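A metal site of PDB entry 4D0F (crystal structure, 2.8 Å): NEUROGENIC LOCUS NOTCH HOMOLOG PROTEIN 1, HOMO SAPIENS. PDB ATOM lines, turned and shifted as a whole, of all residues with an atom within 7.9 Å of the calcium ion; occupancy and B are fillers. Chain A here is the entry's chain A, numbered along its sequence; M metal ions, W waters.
The side-chain hydroxyl (OG1) of Thr 24 sits close to the backbone NH (N) of Ser 27, at 3.4 Å. The side-chain hydroxyl of Thr 24 lies within hydrogen-bond range of the backbone NH of Phe 28 (3.4 Å). SG of Cys 8 lies within hydrogen-bond range of N of Asn 23 (3.6 Å).
Merely in contact with the calcium ion: Gly 26. Within 4 Å of the calcium ion: Val 5, Glu 7, Asn 23, Thr 24, Gly 26 and Ser 27.
The calcium ion is bound by O of Ser 27 (2.3 Å), O of Thr 24 (2.4 Å), OE1 of Glu 7 (2.4 Å), O of Val 5 (2.5 Å) and OD1 of Asn 23 (2.8 Å).
Water W1 lies within hydrogen-bond range of the side-chain carboxylate (OD1) of Asp 4 and the backbone NH (N) of Val 5.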
ATOM      1  N   GLN A   3      22.147 -21.841 -11.455  1.00  0.00           N
ATOM      2  CA  GLN A   3      21.994 -20.381 -11.223  1.00  0.00           C
ATOM      3  C   GLN A   3      22.969 -19.565 -12.183  1.00  0.00           C
ATOM      4  O   GLN A   3      24.109 -19.979 -12.371  1.00  0.00           O
ATOM      5  CB  GLN A   3      22.287 -20.072  -9.741  1.00  0.00           C
ATOM      6  CG  GLN A   3      22.614 -18.651  -9.400  1.00  0.00           C
ATOM      7  CD  GLN A   3      21.375 -17.800  -9.284  1.00  0.00           C
ATOM      8  OE1 GLN A   3      20.906 -17.186 -10.260  1.00  0.00           O
ATOM      9  NE2 GLN A   3      20.835 -17.728  -8.062  1.00  0.00           N
ATOM     10  N   ASP A   4      22.532 -18.429 -12.772  1.00  0.00           N
ATOM     11  CA  ASP A   4      23.364 -17.627 -13.702  1.00  0.00           C
ATOM     12  C   ASP A   4      24.280 -16.571 -13.038  1.00  0.00           C
ATOM     13  O   ASP A   4      23.815 -15.502 -12.631  1.00  0.00           O
ATOM     14  CB  ASP A   4      22.514 -17.014 -14.836  1.00  0.00           C
ATOM     15  CG  ASP A   4      23.303 -16.240 -15.882  1.00  0.00           C
ATOM     16  OD1 ASP A   4      24.453 -16.652 -16.197  1.00  0.00           O
ATOM     17  OD2 ASP A   4      22.771 -15.244 -16.389  1.00  0.00           O
ATOM     18  N   VAL A   5      25.600 -16.876 -12.997  1.00  0.00           N
ATOM     19  CA  VAL A   5      26.641 -16.032 -12.370  1.00  0.00           C
ATOM     20  C   VAL A   5      28.000 -16.468 -12.818  1.00  0.00           C
ATOM     21  O   VAL A   5      28.210 -17.660 -13.084  1.00  0.00           O
ATOM     22  CB  VAL A   5      26.544 -15.997 -10.796  1.00  0.00           C
ATOM     23  CG1 VAL A   5      26.741 -17.353 -10.150  1.00  0.00           C
ATOM     24  CG2 VAL A   5      27.467 -14.952 -10.196  1.00  0.00           C
ATOM     25  N   ASP A   6      28.929 -15.518 -12.929  1.00  0.00           N
ATOM     26  CA  ASP A   6      30.300 -15.870 -13.282  1.00  0.00           C
ATOM     27  C   ASP A   6      31.080 -16.086 -11.991  1.00  0.00           C
ATOM     28  O   ASP A   6      31.536 -15.116 -11.372  1.00  0.00           O
ATOM     29  CB  ASP A   6      30.957 -14.788 -14.156  1.00  0.00           C
ATOM     30  CG  ASP A   6      32.386 -15.074 -14.547  1.00  0.00           C
ATOM     31  OD1 ASP A   6      32.945 -16.119 -14.074  1.00  0.00           O
ATOM     32  OD2 ASP A   6      32.934 -14.288 -15.328  1.00  0.00           O
ATOM     33  N   GLU A   7      31.246 -17.359 -11.602  1.00  0.00           N
ATOM     34  CA  GLU A   7      31.941 -17.696 -10.355  1.00  0.00           C
ATOM     35  C   GLU A   7      33.420 -17.299 -10.375  1.00  0.00           C
ATOM     36  O   GLU A   7      34.040 -17.162  -9.317  1.00  0.00           O
ATOM     37  CB  GLU A   7      31.794 -19.175 -10.001  1.00  0.00           C
ATOM     38  CG  GLU A   7      30.375 -19.601  -9.657  1.00  0.00           C
ATOM     39  CD  GLU A   7      29.517 -20.047 -10.824  1.00  0.00           C
ATOM     40  OE1 GLU A   7      29.878 -19.782 -11.990  1.00  0.00           O
ATOM     41  OE2 GLU A   7      28.440 -20.648 -10.563  1.00  0.00           O
ATOM     42  N   CYS A   8      33.968 -17.094 -11.585  1.00  0.00           N
ATOM     43  CA  CYS A   8      35.365 -16.728 -11.754  1.00  0.00           C
ATOM     44  C   CYS A   8      35.585 -15.227 -11.534  1.00  0.00           C
ATOM     45  O   CYS A   8      36.739 -14.819 -11.431  1.00  0.00           O
ATOM     46  CB  CYS A   8      35.876 -17.188 -13.112  1.00  0.00           C
ATOM     47  SG  CYS A   8      35.511 -18.924 -13.503  1.00  0.00           S
ATOM     48  N   ILE A  22      37.258 -21.181 -15.412  1.00  0.00           N
ATOM     49  CA  ILE A  22      36.540 -21.027 -16.664  1.00  0.00           C
ATOM     50  C   ILE A  22      35.054 -21.036 -16.369  1.00  0.00           C
ATOM     51  O   ILE A  22      34.529 -22.016 -15.823  1.00  0.00           O
ATOM     52  CB  ILE A  22      36.978 -22.098 -17.698  1.00  0.00           C
ATOM     53  CG1 ILE A  22      38.439 -21.834 -18.162  1.00  0.00           C
ATOM     54  CG2 ILE A  22      36.012 -22.129 -18.901  1.00  0.00           C
ATOM     55  CD1 ILE A  22      39.121 -22.973 -18.795  1.00  0.00           C
ATOM     56  N   ASN A  23      34.372 -19.973 -16.723  1.00  0.00           N
ATOM     57  CA  ASN A  23      32.969 -19.913 -16.412  1.00  0.00           C
ATOM     58  C   ASN A  23      32.121 -20.753 -17.358  1.00  0.00           C
ATOM     59  O   ASN A  23      32.468 -20.881 -18.532  1.00  0.00           O
ATOM     60  CB  ASN A  23      32.497 -18.447 -16.403  1.00  0.00           C
ATOM     61  CG  ASN A  23      31.092 -18.251 -15.935  1.00  0.00           C
ATOM     62  OD1 ASN A  23      30.649 -18.881 -14.972  1.00  0.00           O
ATOM     63  ND2 ASN A  23      30.366 -17.375 -16.601  1.00  0.00           N
ATOM     64  N   THR A  24      31.047 -21.361 -16.827  1.00  0.00           N
ATOM     65  CA  THR A  24      30.002 -22.033 -17.601  1.00  0.00           C
ATOM     66  C   THR A  24      28.625 -21.509 -17.153  1.00  0.00           C
ATOM     67  O   THR A  24      28.506 -20.928 -16.074  1.00  0.00           O
ATOM     68  CB  THR A  24      30.047 -23.555 -17.545  1.00  0.00           C
ATOM     69  OG1 THR A  24      29.545 -24.031 -16.301  1.00  0.00           O
ATOM     70  CG2 THR A  24      31.404 -24.105 -17.817  1.00  0.00           C
ATOM     71  N   LEU A  25      27.586 -21.723 -17.961  1.00  0.00           N
ATOM     72  CA  LEU A  25      26.234 -21.315 -17.591  1.00  0.00           C
ATOM     73  C   LEU A  25      25.727 -22.347 -16.576  1.00  0.00           C
ATOM     74  O   LEU A  25      25.636 -23.544 -16.894  1.00  0.00           O
ATOM     75  CB  LEU A  25      25.333 -21.241 -18.837  1.00  0.00           C
ATOM     76  CG  LEU A  25      23.792 -21.341 -18.660  1.00  0.00           C
ATOM     77  CD1 LEU A  25      23.234 -20.206 -17.770  1.00  0.00           C
ATOM     78  CD2 LEU A  25      23.089 -21.366 -20.021  1.00  0.00           C
ATOM     79  N   GLY A  26      25.465 -21.880 -15.355  1.00  0.00           N
ATOM     80  CA  GLY A  26      25.002 -22.761 -14.285  1.00  0.00           C
ATOM     81  C   GLY A  26      26.087 -23.345 -13.401  1.00  0.00           C
ATOM     82  O   GLY A  26      25.781 -23.913 -12.342  1.00  0.00           O
ATOM     83  N   SER A  27      27.350 -23.253 -13.812  1.00  0.00           N
ATOM     84  CA  SER A  27      28.480 -23.695 -12.987  1.00  0.00           C
ATOM     85  C   SER A  27      29.777 -23.002 -13.442  1.00  0.00           C
ATOM     86  O   SER A  27      29.743 -21.876 -13.944  1.00  0.00           O
ATOM     87  CB  SER A  27      28.622 -25.217 -13.023  1.00  0.00           C
ATOM     88  OG  SER A  27      29.428 -25.685 -11.954  1.00  0.00           O
ATOM     89  N   PHE A  28      30.895 -23.678 -13.232  1.00  0.00           N
ATOM     90  CA  PHE A  28      32.220 -23.260 -13.654  1.00  0.00           C
ATOM     91  C   PHE A  28      33.086 -24.525 -13.707  1.00  0.00           C
ATOM     92  O   PHE A  28      32.698 -25.595 -13.223  1.00  0.00           O
ATOM     93  CB  PHE A  28      32.833 -22.188 -12.723  1.00  0.00           C
ATOM     94  CG  PHE A  28      33.140 -22.683 -11.331  1.00  0.00           C
ATOM     95  CD1 PHE A  28      32.151 -22.699 -10.344  1.00  0.00           C
ATOM     96  CD2 PHE A  28      34.411 -23.118 -10.999  1.00  0.00           C
ATOM     97  CE1 PHE A  28      32.439 -23.132  -9.067  1.00  0.00           C
ATOM     98  CE2 PHE A  28      34.679 -23.574  -9.709  1.00  0.00           C
ATOM     99  CZ  PHE A  28      33.695 -23.572  -8.764  1.00  0.00           C
ATOM    100  N   GLU A  29      34.253 -24.409 -14.352  1.00  0.00           N
ATOM    101  CA  GLU A  29      35.182 -25.508 -14.462  1.00  0.00           C
ATOM    102  C   GLU A  29      36.585 -25.008 -14.195  1.00  0.00           C
ATOM    103  O   GLU A  29      36.900 -23.817 -14.406  1.00  0.00           O
ATOM    104  CB  GLU A  29      35.124 -26.244 -15.805  1.00  0.00           C
ATOM    105  CG  GLU A  29      33.825 -26.173 -16.586  1.00  0.00           C
ATOM    106  CD  GLU A  29      33.956 -26.853 -17.920  1.00  0.00           C
ATOM    107  OE1 GLU A  29      34.271 -28.071 -17.916  1.00  0.00           O
ATOM    108  OE2 GLU A  29      33.805 -26.192 -18.978  1.00  0.00           O
HETATM  109 CA    CA M   1      28.348 -20.056 -13.859  1.00  0.00          CA
HETATM  110  O   HOH W   1      26.977 -17.909 -15.795  1.00  0.00           O
